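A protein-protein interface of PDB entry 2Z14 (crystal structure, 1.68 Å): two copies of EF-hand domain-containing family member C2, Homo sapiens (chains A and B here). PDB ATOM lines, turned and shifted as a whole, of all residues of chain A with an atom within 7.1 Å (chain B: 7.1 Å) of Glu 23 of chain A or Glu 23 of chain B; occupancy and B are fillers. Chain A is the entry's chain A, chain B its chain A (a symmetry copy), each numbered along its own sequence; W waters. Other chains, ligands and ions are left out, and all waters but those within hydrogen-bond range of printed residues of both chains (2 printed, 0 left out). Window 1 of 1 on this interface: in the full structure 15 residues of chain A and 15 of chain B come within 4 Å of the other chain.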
ATOM      1  N   TYR A  21       0.374 -21.338  37.021  1.00  0.00           N
ATOM      2  CA  TYR A  21       0.590 -19.976  36.562  1.00  0.00           C
ATOM      3  C   TYR A  21      -0.750 -19.400  36.171  1.00  0.00           C
ATOM      4  O   TYR A  21      -1.739 -20.116  36.041  1.00  0.00           O
ATOM      5  CB  TYR A  21       1.538 -19.943  35.351  1.00  0.00           C
ATOM      6  CG  TYR A  21       0.926 -20.406  34.039  1.00  0.00           C
ATOM      7  CD1 TYR A  21       0.331 -19.496  33.159  1.00  0.00           C
ATOM      8  CD2 TYR A  21       0.938 -21.751  33.681  1.00  0.00           C
ATOM      9  CE1 TYR A  21      -0.233 -19.920  31.953  1.00  0.00           C
ATOM     10  CE2 TYR A  21       0.376 -22.185  32.481  1.00  0.00           C
ATOM     11  CZ  TYR A  21      -0.204 -21.266  31.623  1.00  0.00           C
ATOM     12  OH  TYR A  21      -0.745 -21.687  30.429  1.00  0.00           O
ATOM     13  N   LEU A  22      -0.785 -18.089  36.021  1.00  0.00           N
ATOM     14  CA  LEU A  22      -1.995 -17.420  35.590  1.00  0.00           C
ATOM     15  C   LEU A  22      -1.536 -16.153  34.918  1.00  0.00           C
ATOM     16  O   LEU A  22      -0.410 -15.697  35.128  1.00  0.00           O
ATOM     17  CB  LEU A  22      -2.924 -17.101  36.772  1.00  0.00           C
ATOM     18  CG  LEU A  22      -2.485 -16.180  37.916  1.00  0.00           C
ATOM     19  CD1 LEU A  22      -2.318 -14.748  37.429  1.00  0.00           C
ATOM     20  CD2 LEU A  22      -3.543 -16.226  39.012  1.00  0.00           C
ATOM     21  N   GLU A  23      -2.388 -15.608  34.069  1.00  0.00           N
ATOM     22  CA  GLU A  23      -2.053 -14.373  33.407  1.00  0.00           C
ATOM     23  C   GLU A  23      -2.874 -13.296  34.077  1.00  0.00           C
ATOM     24  O   GLU A  23      -4.087 -13.440  34.244  1.00  0.00           O
ATOM     25  CB  GLU A  23      -2.391 -14.429  31.913  1.00  0.00           C
ATOM     26  CG  GLU A  23      -1.502 -15.355  31.099  1.00  0.00           C
ATOM     27  CD  GLU A  23      -2.211 -16.619  30.659  1.00  0.00           C
ATOM     28  OE1 GLU A  23      -3.402 -16.787  30.990  1.00  0.00           O
ATOM     29  OE2 GLU A  23      -1.577 -17.448  29.977  1.00  0.00           O
ATOM     30  N   GLU A  24      -2.200 -12.242  34.511  1.00  0.00           N
ATOM     31  CA  GLU A  24      -2.882 -11.113  35.109  1.00  0.00           C
ATOM     32  C   GLU A  24      -3.164 -10.272  33.872  1.00  0.00           C
ATOM     33  O   GLU A  24      -2.255  -9.696  33.278  1.00  0.00           O
ATOM     34  CB  GLU A  24      -1.964 -10.378  36.084  1.00  0.00           C
ATOM     35  CG  GLU A  24      -2.525  -9.048  36.560  1.00  0.00           C
ATOM     36  CD  GLU A  24      -1.955  -8.613  37.893  1.00  0.00           C
ATOM     37  OE1 GLU A  24      -0.732  -8.755  38.094  1.00  0.00           O
ATOM     38  OE2 GLU A  24      -2.734  -8.120  38.740  1.00  0.00           O
ATOM     39  N   GLU A  25      -4.425 -10.254  33.466  1.00  0.00           N
ATOM     40  CA  GLU A  25      -4.838  -9.541  32.270  1.00  0.00           C
ATOM     41  C   GLU A  25      -5.566  -8.251  32.597  1.00  0.00           C
ATOM     42  O   GLU A  25      -6.691  -8.269  33.097  1.00  0.00           O
ATOM     43  CB  GLU A  25      -5.722 -10.458  31.432  1.00  0.00           C
ATOM     44  CG  GLU A  25      -5.063 -11.797  31.155  1.00  0.00           C
ATOM     45  CD  GLU A  25      -6.005 -12.805  30.545  1.00  0.00           C
ATOM     46  OE1 GLU A  25      -6.958 -13.226  31.234  1.00  0.00           O
ATOM     47  OE2 GLU A  25      -5.792 -13.174  29.375  1.00  0.00           O
ATOM     48  N   VAL A  26      -4.911  -7.132  32.306  1.00  0.00           N
ATOM     49  CA  VAL A  26      -5.475  -5.818  32.573  1.00  0.00           C
ATOM     50  C   VAL A  26      -6.078  -5.215  31.309  1.00  0.00           C
ATOM     51  O   VAL A  26      -5.386  -4.989  30.312  1.00  0.00           O
ATOM     52  CB  VAL A  26      -4.401  -4.866  33.149  1.00  0.00           C
ATOM     53  CG1 VAL A  26      -5.006  -3.506  33.444  1.00  0.00           C
ATOM     54  CG2 VAL A  26      -3.811  -5.466  34.422  1.00  0.00           C
ATOM     55  N   ASN A  33      -3.443  -5.953  28.174  1.00  0.00           N
ATOM     56  CA  ASN A  33      -2.035  -6.214  28.409  1.00  0.00           C
ATOM     57  C   ASN A  33      -2.009  -7.290  29.480  1.00  0.00           C
ATOM     58  O   ASN A  33      -2.995  -7.481  30.191  1.00  0.00           O
ATOM     59  CB  ASN A  33      -1.325  -4.955  28.905  1.00  0.00           C
ATOM     60  CG  ASN A  33      -1.251  -3.882  27.845  1.00  0.00           C
ATOM     61  OD1 ASN A  33      -0.703  -4.100  26.765  1.00  0.00           O
ATOM     62  ND2 ASN A  33      -1.803  -2.713  28.146  1.00  0.00           N
ATOM     63  N   TYR A  34      -0.896  -7.998  29.602  1.00  0.00           N
ATOM     64  CA  TYR A  34      -0.830  -9.056  30.593  1.00  0.00           C
ATOM     65  C   TYR A  34       0.592  -9.359  31.023  1.00  0.00           C
ATOM     66  O   TYR A  34       1.564  -8.945  30.389  1.00  0.00           O
ATOM     67  CB  TYR A  34      -1.433 -10.345  30.011  1.00  0.00           C
ATOM     68  CG  TYR A  34      -0.461 -11.095  29.115  1.00  0.00           C
ATOM     69  CD1 TYR A  34       0.317 -12.142  29.618  1.00  0.00           C
ATOM     70  CD2 TYR A  34      -0.248 -10.694  27.795  1.00  0.00           C
ATOM     71  CE1 TYR A  34       1.291 -12.766  28.829  1.00  0.00           C
ATOM     72  CE2 TYR A  34       0.721 -11.310  27.000  1.00  0.00           C
ATOM     73  CZ  TYR A  34       1.490 -12.341  27.525  1.00  0.00           C
ATOM     74  OH  TYR A  34       2.468 -12.933  26.755  1.00  0.00           O
ATOM     75  N   ARG A  35       0.695 -10.090  32.122  1.00  0.00           N
ATOM     76  CA  ARG A  35       1.977 -10.546  32.618  1.00  0.00           C
ATOM     77  C   ARG A  35       1.683 -11.923  33.185  1.00  0.00           C
ATOM     78  O   ARG A  35       0.535 -12.230  33.516  1.00  0.00           O
ATOM     79  CB  ARG A  35       2.546  -9.597  33.679  1.00  0.00           C
ATOM     80  CG  ARG A  35       1.907  -9.630  35.058  1.00  0.00           C
ATOM     81  CD  ARG A  35       2.432  -8.444  35.861  1.00  0.00           C
ATOM     82  NE  ARG A  35       2.223  -8.559  37.300  1.00  0.00           N
ATOM     83  CZ  ARG A  35       3.016  -9.241  38.123  1.00  0.00           C
ATOM     84  NH1 ARG A  35       4.080  -9.877  37.653  1.00  0.00           N
ATOM     85  NH2 ARG A  35       2.754  -9.273  39.423  1.00  0.00           N
ATOM     86  N   ILE A  36       2.699 -12.769  33.255  1.00  0.00           N
ATOM     87  CA  ILE A  36       2.507 -14.112  33.783  1.00  0.00           C
ATOM     88  C   ILE A  36       3.011 -14.161  35.215  1.00  0.00           C
ATOM     89  O   ILE A  36       4.078 -13.633  35.527  1.00  0.00           O
ATOM     90  CB  ILE A  36       3.268 -15.155  32.944  1.00  0.00           C
ATOM     91  CG1 ILE A  36       2.849 -15.048  31.476  1.00  0.00           C
ATOM     92  CG2 ILE A  36       2.976 -16.565  33.473  1.00  0.00           C
ATOM     93  CD1 ILE A  36       3.629 -15.969  30.554  1.00  0.00           C
ATOM     94  N   ARG A  37       2.226 -14.777  36.089  1.00  0.00           N
ATOM     95  CA  ARG A  37       2.611 -14.902  37.485  1.00  0.00           C
ATOM     96  C   ARG A  37       2.614 -16.380  37.832  1.00  0.00           C
ATOM     97  O   ARG A  37       1.706 -17.122  37.447  1.00  0.00           O
ATOM     98  CB  ARG A  37       1.649 -14.101  38.362  1.00  0.00           C
ATOM     99  CG  ARG A  37       1.735 -12.607  38.055  1.00  0.00           C
ATOM    100  CD  ARG A  37       0.809 -11.758  38.902  1.00  0.00           C
ATOM    101  NE  ARG A  37       1.202 -11.730  40.307  1.00  0.00           N
ATOM    102  CZ  ARG A  37       0.639 -10.941  41.217  1.00  0.00           C
ATOM    103  NH1 ARG A  37      -0.337 -10.112  40.862  1.00  0.00           N
ATOM    104  NH2 ARG A  37       1.038 -10.991  42.480  1.00  0.00           N
ATOM    105  N   TYR A  39       2.764 -19.538  40.598  1.00  0.00           N
ATOM    106  CA  TYR A  39       2.378 -19.912  41.944  1.00  0.00           C
ATOM    107  C   TYR A  39       2.623 -21.367  42.282  1.00  0.00           C
ATOM    108  O   TYR A  39       2.719 -22.229  41.408  1.00  0.00           O
ATOM    109  CB  TYR A  39       0.888 -19.648  42.161  1.00  0.00           C
ATOM    110  CG  TYR A  39       0.464 -18.220  41.966  1.00  0.00           C
ATOM    111  CD1 TYR A  39       0.216 -17.708  40.692  1.00  0.00           C
ATOM    112  CD2 TYR A  39       0.292 -17.380  43.062  1.00  0.00           C
ATOM    113  CE1 TYR A  39      -0.195 -16.389  40.518  1.00  0.00           C
ATOM    114  CE2 TYR A  39      -0.119 -16.067  42.902  1.00  0.00           C
ATOM    115  CZ  TYR A  39      -0.361 -15.577  41.629  1.00  0.00           C
ATOM    116  OH  TYR A  39      -0.777 -14.276  41.480  1.00  0.00           O
ATOM    117  N   GLU A  94      -7.182 -26.942  35.006  1.00  0.00           N
ATOM    118  CA  GLU A  94      -7.341 -25.589  35.517  1.00  0.00           C
ATOM    119  C   GLU A  94      -8.199 -25.634  36.769  1.00  0.00           C
ATOM    120  O   GLU A  94      -9.118 -26.447  36.873  1.00  0.00           O
ATOM    121  CB  GLU A  94      -8.022 -24.687  34.481  1.00  0.00           C
ATOM    122  CG  GLU A  94      -7.362 -24.682  33.114  1.00  0.00           C
ATOM    123  CD  GLU A  94      -7.929 -23.613  32.201  1.00  0.00           C
ATOM    124  OE1 GLU A  94      -9.076 -23.172  32.438  1.00  0.00           O
ATOM    125  OE2 GLU A  94      -7.233 -23.225  31.238  1.00  0.00           O
ATOM    126  N   ARG A 100     -10.343 -16.475  39.944  1.00  0.00           N
ATOM    127  CA  ARG A 100      -9.146 -16.488  39.111  1.00  0.00           C
ATOM    128  C   ARG A 100      -8.769 -17.900  38.682  1.00  0.00           C
ATOM    129  O   ARG A 100      -8.788 -18.838  39.482  1.00  0.00           O
ATOM    130  CB  ARG A 100      -7.983 -15.810  39.841  1.00  0.00           C
ATOM    131  CG  ARG A 100      -8.242 -14.332  40.159  1.00  0.00           C
ATOM    132  CD  ARG A 100      -8.692 -13.556  38.919  1.00  0.00           C
ATOM    133  NE  ARG A 100      -8.949 -12.144  39.209  1.00  0.00           N
ATOM    134  CZ  ARG A 100      -9.462 -11.278  38.338  1.00  0.00           C
ATOM    135  NH1 ARG A 100      -9.660 -10.014  38.692  1.00  0.00           N
ATOM    136  NH2 ARG A 100      -9.785 -11.672  37.114  1.00  0.00           N
ATOM    137  N   THR A 101      -8.430 -18.037  37.406  1.00  0.00           N
ATOM    138  CA  THR A 101      -8.076 -19.327  36.825  1.00  0.00           C
ATOM    139  C   THR A 101      -6.590 -19.661  36.893  1.00  0.00           C
ATOM    140  O   THR A 101      -5.762 -18.994  36.269  1.00  0.00           O
ATOM    141  CB  THR A 101      -8.518 -19.390  35.353  1.00  0.00           C
ATOM    142  OG1 THR A 101      -9.937 -19.215  35.274  1.00  0.00           O
ATOM    143  CG2 THR A 101      -8.142 -20.734  34.738  1.00  0.00           C
ATOM    144  N   LYS A 103      -3.602 -22.276  36.079  1.00  0.00           N
ATOM    145  CA  LYS A 103      -3.268 -23.357  35.159  1.00  0.00           C
ATOM    146  C   LYS A 103      -2.112 -24.177  35.729  1.00  0.00           C
ATOM    147  O   LYS A 103      -0.987 -23.691  35.846  1.00  0.00           O
ATOM    148  CB  LYS A 103      -2.909 -22.768  33.794  1.00  0.00           C
ATOM    149  CG  LYS A 103      -4.116 -22.162  33.093  1.00  0.00           C
ATOM    150  CD  LYS A 103      -3.761 -20.948  32.264  1.00  0.00           C
ATOM    151  CE  LYS A 103      -5.022 -20.329  31.681  1.00  0.00           C
ATOM    152  NZ  LYS A 103      -4.790 -18.961  31.154  1.00  0.00           N
ATOM    153  N   TYR B  21       1.698 -17.328  22.358  1.00  0.00           N
ATOM    154  CA  TYR B  21       1.209 -18.620  22.811  1.00  0.00           C
ATOM    155  C   TYR B  21      -0.256 -18.469  23.148  1.00  0.00           C
ATOM    156  O   TYR B  21      -0.777 -17.361  23.249  1.00  0.00           O
ATOM    157  CB  TYR B  21       1.977 -19.097  24.056  1.00  0.00           C
ATOM    158  CG  TYR B  21       1.620 -18.383  25.349  1.00  0.00           C
ATOM    159  CD1 TYR B  21       0.626 -18.881  26.198  1.00  0.00           C
ATOM    160  CD2 TYR B  21       2.270 -17.209  25.720  1.00  0.00           C
ATOM    161  CE1 TYR B  21       0.295 -18.225  27.386  1.00  0.00           C
ATOM    162  CE2 TYR B  21       1.945 -16.546  26.903  1.00  0.00           C
ATOM    163  CZ  TYR B  21       0.961 -17.060  27.731  1.00  0.00           C
ATOM    164  OH  TYR B  21       0.650 -16.418  28.908  1.00  0.00           O
ATOM    165  N   LEU B  22      -0.928 -19.596  23.284  1.00  0.00           N
ATOM    166  CA  LEU B  22      -2.325 -19.589  23.664  1.00  0.00           C
ATOM    167  C   LEU B  22      -2.564 -20.914  24.341  1.00  0.00           C
ATOM    168  O   LEU B  22      -1.794 -21.861  24.168  1.00  0.00           O
ATOM    169  CB  LEU B  22      -3.249 -19.429  22.446  1.00  0.00           C
ATOM    170  CG  LEU B  22      -3.270 -20.458  21.310  1.00  0.00           C
ATOM    171  CD1 LEU B  22      -3.838 -21.787  21.790  1.00  0.00           C
ATOM    172  CD2 LEU B  22      -4.132 -19.915  20.177  1.00  0.00           C
ATOM    173  N   GLU B  23      -3.603 -20.969  25.153  1.00  0.00           N
ATOM    174  CA  GLU B  23      -3.934 -22.205  25.816  1.00  0.00           C
ATOM    175  C   GLU B  23      -5.150 -22.754  25.106  1.00  0.00           C
ATOM    176  O   GLU B  23      -6.134 -22.041  24.896  1.00  0.00           O
ATOM    177  CB  GLU B  23      -4.258 -21.977  27.297  1.00  0.00           C
ATOM    178  CG  GLU B  23      -3.061 -21.593  28.151  1.00  0.00           C
ATOM    179  CD  GLU B  23      -3.083 -20.139  28.577  1.00  0.00           C
ATOM    180  OE1 GLU B  23      -4.029 -19.417  28.204  1.00  0.00           O
ATOM    181  OE2 GLU B  23      -2.151 -19.715  29.289  1.00  0.00           O
ATOM    182  N   GLU B  24      -5.057 -24.007  24.687  1.00  0.00           N
ATOM    183  CA  GLU B  24      -6.179 -24.669  24.054  1.00  0.00           C
ATOM    184  C   GLU B  24      -6.879 -25.255  25.271  1.00  0.00           C
ATOM    185  O   GLU B  24      -6.386 -26.194  25.893  1.00  0.00           O
ATOM    186  CB  GLU B  24      -5.699 -25.766  23.105  1.00  0.00           C
ATOM    187  CG  GLU B  24      -6.818 -26.660  22.597  1.00  0.00           C
ATOM    188  CD  GLU B  24      -6.482 -27.330  21.282  1.00  0.00           C
ATOM    189  OE1 GLU B  24      -5.338 -27.801  21.127  1.00  0.00           O
ATOM    190  OE2 GLU B  24      -7.371 -27.391  20.402  1.00  0.00           O
ATOM    191  N   GLU B  25      -8.004 -24.655  25.630  1.00  0.00           N
ATOM    192  CA  GLU B  25      -8.755 -25.067  26.804  1.00  0.00           C
ATOM    193  C   GLU B  25     -10.005 -25.844  26.439  1.00  0.00           C
ATOM    194  O   GLU B  25     -10.961 -25.286  25.898  1.00  0.00           O
ATOM    195  CB  GLU B  25      -9.113 -23.827  27.618  1.00  0.00           C
ATOM    196  CG  GLU B  25      -7.896 -22.974  27.931  1.00  0.00           C
ATOM    197  CD  GLU B  25      -8.253 -21.630  28.516  1.00  0.00           C
ATOM    198  OE1 GLU B  25      -8.855 -20.805  27.797  1.00  0.00           O
ATOM    199  OE2 GLU B  25      -7.930 -21.399  29.697  1.00  0.00           O
ATOM    200  N   VAL B  26      -9.986 -27.137  26.743  1.00  0.00           N
ATOM    201  CA  VAL B  26     -11.108 -28.014  26.443  1.00  0.00           C
ATOM    202  C   VAL B  26     -11.973 -28.237  27.678  1.00  0.00           C
ATOM    203  O   VAL B  26     -11.515 -28.761  28.698  1.00  0.00           O
ATOM    204  CB  VAL B  26     -10.610 -29.373  25.898  1.00  0.00           C
ATOM    205  CG1 VAL B  26     -11.788 -30.272  25.568  1.00  0.00           C
ATOM    206  CG2 VAL B  26      -9.758 -29.148  24.653  1.00  0.00           C
ATOM    207  N   ASN B  33      -9.427 -28.841  30.914  1.00  0.00           N
ATOM    208  CA  ASN B  33      -8.062 -29.299  30.733  1.00  0.00           C
ATOM    209  C   ASN B  33      -7.478 -28.381  29.674  1.00  0.00           C
ATOM    210  O   ASN B  33      -8.221 -27.743  28.929  1.00  0.00           O
ATOM    211  CB  ASN B  33      -8.035 -30.749  30.252  1.00  0.00           C
ATOM    212  CG  ASN B  33      -8.530 -31.713  31.304  1.00  0.00           C
ATOM    213  OD1 ASN B  33      -7.985 -31.779  32.405  1.00  0.00           O
ATOM    214  ND2 ASN B  33      -9.569 -32.470  30.971  1.00  0.00           N
ATOM    215  N   TYR B  34      -6.158 -28.304  29.600  1.00  0.00           N
ATOM    216  CA  TYR B  34      -5.550 -27.420  28.622  1.00  0.00           C
ATOM    217  C   TYR B  34      -4.146 -27.850  28.246  1.00  0.00           C
ATOM    218  O   TYR B  34      -3.521 -28.677  28.912  1.00  0.00           O
ATOM    219  CB  TYR B  34      -5.473 -25.995  29.194  1.00  0.00           C
ATOM    220  CG  TYR B  34      -4.292 -25.803  30.131  1.00  0.00           C
ATOM    221  CD1 TYR B  34      -3.086 -25.270  29.667  1.00  0.00           C
ATOM    222  CD2 TYR B  34      -4.349 -26.244  31.454  1.00  0.00           C
ATOM    223  CE1 TYR B  34      -1.961 -25.189  30.497  1.00  0.00           C
ATOM    224  CE2 TYR B  34      -3.232 -26.169  32.289  1.00  0.00           C
ATOM    225  CZ  TYR B  34      -2.041 -25.645  31.803  1.00  0.00           C
ATOM    226  OH  TYR B  34      -0.927 -25.596  32.613  1.00  0.00           O
ATOM    227  N   ARG B  35      -3.661 -27.271  27.159  1.00  0.00           N
ATOM    228  CA  ARG B  35      -2.302 -27.499  26.715  1.00  0.00           C
ATOM    229  C   ARG B  35      -1.869 -26.158  26.150  1.00  0.00           C
ATOM    230  O   ARG B  35      -2.710 -25.335  25.780  1.00  0.00           O
ATOM    231  CB  ARG B  35      -2.226 -28.615  25.666  1.00  0.00           C
ATOM    232  CG  ARG B  35      -2.718 -28.289  24.264  1.00  0.00           C
ATOM    233  CD  ARG B  35      -2.806 -29.588  23.470  1.00  0.00           C
ATOM    234  NE  ARG B  35      -2.881 -29.399  22.026  1.00  0.00           N
ATOM    235  CZ  ARG B  35      -1.827 -29.197  21.239  1.00  0.00           C
ATOM    236  NH1 ARG B  35      -0.605 -29.153  21.753  1.00  0.00           N
ATOM    237  NH2 ARG B  35      -1.993 -29.053  19.930  1.00  0.00           N
ATOM    238  N   ILE B  36      -0.568 -25.913  26.125  1.00  0.00           N
ATOM    239  CA  ILE B  36      -0.065 -24.650  25.603  1.00  0.00           C
ATOM    240  C   ILE B  36       0.452 -24.866  24.190  1.00  0.00           C
ATOM    241  O   ILE B  36       1.139 -25.848  23.913  1.00  0.00           O
ATOM    242  CB  ILE B  36       1.076 -24.100  26.479  1.00  0.00           C
ATOM    243  CG1 ILE B  36       0.605 -23.976  27.930  1.00  0.00           C
ATOM    244  CG2 ILE B  36       1.525 -22.730  25.953  1.00  0.00           C
ATOM    245  CD1 ILE B  36       1.699 -23.541  28.888  1.00  0.00           C
ATOM    246  N   ARG B  37       0.097 -23.954  23.295  1.00  0.00           N
ATOM    247  CA  ARG B  37       0.545 -24.045  21.915  1.00  0.00           C
ATOM    248  C   ARG B  37       1.277 -22.757  21.582  1.00  0.00           C
ATOM    249  O   ARG B  37       0.830 -21.665  21.941  1.00  0.00           O
ATOM    250  CB  ARG B  37      -0.652 -24.287  20.995  1.00  0.00           C
ATOM    251  CG  ARG B  37      -1.314 -25.631  21.291  1.00  0.00           C
ATOM    252  CD  ARG B  37      -2.504 -25.933  20.404  1.00  0.00           C
ATOM    253  NE  ARG B  37      -2.123 -26.161  19.013  1.00  0.00           N
ATOM    254  CZ  ARG B  37      -2.965 -26.585  18.077  1.00  0.00           C
ATOM    255  NH1 ARG B  37      -4.233 -26.834  18.387  1.00  0.00           N
ATOM    256  NH2 ARG B  37      -2.546 -26.748  16.829  1.00  0.00           N
ATOM    257  N   TYR B  39       3.042 -20.096  18.853  1.00  0.00           N
ATOM    258  CA  TYR B  39       2.936 -19.595  17.498  1.00  0.00           C
ATOM    259  C   TYR B  39       3.868 -18.445  17.182  1.00  0.00           C
ATOM    260  O   TYR B  39       4.339 -17.730  18.068  1.00  0.00           O
ATOM    261  CB  TYR B  39       1.514 -19.104  17.224  1.00  0.00           C
ATOM    262  CG  TYR B  39       0.443 -20.144  17.390  1.00  0.00           C
ATOM    263  CD1 TYR B  39      -0.069 -20.460  18.650  1.00  0.00           C
ATOM    264  CD2 TYR B  39      -0.075 -20.806  16.280  1.00  0.00           C
ATOM    265  CE1 TYR B  39      -1.074 -21.412  18.796  1.00  0.00           C
ATOM    266  CE2 TYR B  39      -1.077 -21.752  16.414  1.00  0.00           C
ATOM    267  CZ  TYR B  39      -1.573 -22.052  17.672  1.00  0.00           C
ATOM    268  OH  TYR B  39      -2.573 -22.985  17.794  1.00  0.00           O
ATOM    269  N   GLU B  94      -2.254  -8.742  24.149  1.00  0.00           N
ATOM    270  CA  GLU B  94      -3.032  -9.853  23.620  1.00  0.00           C
ATOM    271  C   GLU B  94      -3.714  -9.409  22.338  1.00  0.00           C
ATOM    272  O   GLU B  94      -4.118  -8.253  22.208  1.00  0.00           O
ATOM    273  CB  GLU B  94      -4.103 -10.300  24.621  1.00  0.00           C
ATOM    274  CG  GLU B  94      -3.578 -10.612  26.012  1.00  0.00           C
ATOM    275  CD  GLU B  94      -4.626 -11.263  26.894  1.00  0.00           C
ATOM    276  OE1 GLU B  94      -5.833 -11.094  26.611  1.00  0.00           O
ATOM    277  OE2 GLU B  94      -4.241 -11.931  27.877  1.00  0.00           O
ATOM    278  N   ARG B 100      -9.918 -16.404  19.001  1.00  0.00           N
ATOM    279  CA  ARG B 100      -8.896 -16.966  19.877  1.00  0.00           C
ATOM    280  C   ARG B 100      -7.897 -15.910  20.332  1.00  0.00           C
ATOM    281  O   ARG B 100      -7.429 -15.089  19.541  1.00  0.00           O
ATOM    282  CB  ARG B 100      -8.182 -18.130  19.183  1.00  0.00           C
ATOM    283  CG  ARG B 100      -9.115 -19.299  18.842  1.00  0.00           C
ATOM    284  CD  ARG B 100      -9.930 -19.748  20.057  1.00  0.00           C
ATOM    285  NE  ARG B 100     -10.830 -20.860  19.745  1.00  0.00           N
ATOM    286  CZ  ARG B 100     -11.730 -21.360  20.588  1.00  0.00           C
ATOM    287  NH1 ARG B 100     -12.503 -22.372  20.215  1.00  0.00           N
ATOM    288  NH2 ARG B 100     -11.865 -20.847  21.804  1.00  0.00           N
ATOM    289  N   THR B 101      -7.580 -15.943  21.621  1.00  0.00           N
ATOM    290  CA  THR B 101      -6.666 -14.982  22.227  1.00  0.00           C
ATOM    291  C   THR B 101      -5.204 -15.412  22.217  1.00  0.00           C
ATOM    292  O   THR B 101      -4.826 -16.391  22.864  1.00  0.00           O
ATOM    293  CB  THR B 101      -7.076 -14.699  23.682  1.00  0.00           C
ATOM    294  OG1 THR B 101      -8.403 -14.162  23.708  1.00  0.00           O
ATOM    295  CG2 THR B 101      -6.117 -13.701  24.323  1.00  0.00           C
ATOM    296  N   LYS B 103      -1.354 -14.570  23.163  1.00  0.00           N
ATOM    297  CA  LYS B 103      -0.571 -13.778  24.104  1.00  0.00           C
ATOM    298  C   LYS B 103       0.858 -13.627  23.585  1.00  0.00           C
ATOM    299  O   LYS B 103       1.609 -14.599  23.504  1.00  0.00           O
ATOM    300  CB  LYS B 103      -0.593 -14.454  25.476  1.00  0.00           C
ATOM    301  CG  LYS B 103      -1.967 -14.391  26.127  1.00  0.00           C
ATOM    302  CD  LYS B 103      -2.276 -15.617  26.958  1.00  0.00           C
ATOM    303  CE  LYS B 103      -3.700 -15.540  27.488  1.00  0.00           C
ATOM    304  NZ  LYS B 103      -4.180 -16.844  28.010  1.00  0.00           N
HETATM  305  O   HOH W   1      -7.384 -18.903  30.220  1.00  0.00           O
HETATM  306  O   HOH W   2      -6.508 -15.627  28.849  1.00  0.00           O
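The side-chain hydroxyl (OH) of Tyr 21 of chain A sits at hydrogen-bond distance from the side-chain carboxylate (OE2) of Glu 23 of chain B, at 2.7 Å. The side-chain hydroxyl (OH) of Tyr 21 of chain B sits at hydrogen-bond distance from the side-chain carboxylate (OE2) of Glu 23 of chain A (2.7 Å). The side-chain carboxylate (OE2) of Glu 23 of chain A sits close to the side-chain carboxylate (OE2) of Glu 23 of chain B, at 2.4 Å. The side-chain amino group (NZ) of Lys 103 of chain B is in salt-bridge range of the side-chain carboxylate (OE1) of Glu 23 of chain A (3.1 Å). OE2 of Glu 25 of chain A sits close to OE2 of Glu 94 of chain B, 2.5 Å away. The side-chain carboxylate (OE2) of Glu 25 of chain B lies close to the side-chain carboxylate (OE2) of Glu 94 of chain A (2.5 Å). The side-chain amino group (NZ) of Lys 103 of chain A lies within salt-bridge range of the side-chain carboxylate (OE1) of Glu 23 of chain B (3.1 Å).
The backbone carbonyl oxygen (O) of Tyr 21 of chain A sits at hydrogen-bond distance from the backbone NH (N) of Lys 103 of chain A (2.9 Å). The side-chain carboxylate (OE1) of Glu 23 of chain A is in salt-bridge range of the side-chain amino group (NZ) of Lys 103 of chain A, 2.6 Å away. OE1 of Glu 23 of chain B lies within salt-bridge range of NZ of Lys 103 of chain B (2.6 Å).
Among the printed residues, pairs that only touch across the chains: Tyr 21 of chain A with Tyr 34 of chain B, Tyr 21 of chain A with Ile 36 of chain B, Glu 25 of chain A with Lys 103 of chain B, Tyr 34 of chain A with Tyr 21 of chain B, Tyr 34 of chain A with Glu 94 of chain B, Tyr 34 of chain A with Lys 103 of chain B, Ile 36 of chain A with Tyr 21 of chain B, Glu 94 of chain A with Tyr 34 of chain B, Lys 103 of chain A with Glu 25 of chain B, Lys 103 of chain A with Tyr 34 of chain B and Lys 103 of chain A with Lys 103 of chain B.
Of the printed residues of chain B, Glu 23 of chain A touches Tyr 21 (2.7 Å), Glu 23 (2.4 Å) and Lys 103 (3.1 Å). Of the printed residues of chain B, Ile 36 of chain A touches Tyr 21. Printed residues of chain A within 4 Å of Tyr 34 of chain B: Tyr 21, Glu 94 and Lys 103. Tyr 39 of chain B touches none of the printed residues of chain A. The nearest residue of chain A that does not touch Glu 23 of chain B is Glu 94 of chain A (5.1 Å). The nearest printed residue of chain A that does not touch Tyr 34 of chain B is Thr 101 of chain A (7.5 Å).
Of the 16 printed residues of chain A, 7 touch a printed residue of chain B. Among the printed residues, Asp or Glu carboxylates within 4 Å of a Lys or Arg side-chain nitrogen of the other chain: Glu 23 of chain A with Lys 103 of chain B and Lys 103 of chain A with Glu 23 of chain B.
Tyr 21 of chain A touches Glu 23 of chain B, and with the chains exchanged Glu 23 of chain A touches Tyr 21 of chain B. Tyr 21 of chain A touches Tyr 34 of chain B, and with the chains exchanged Tyr 34 of chain A touches Tyr 21 of chain B. Positions printed for both chains: 21, 22, 23, 24, 25, 26, 33, 34, 35, 36, 37, 39, 94, 100, 101 and 103.
Water W1 bridges OE2 of Glu 25 of chain B (2.6 Å) and NZ of Lys 103 of chain A (2.8 Å). Water W2 bridges OE2 of Glu 25 of chain A (2.6 Å) and NZ of Lys 103 of chain B (2.8 Å).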
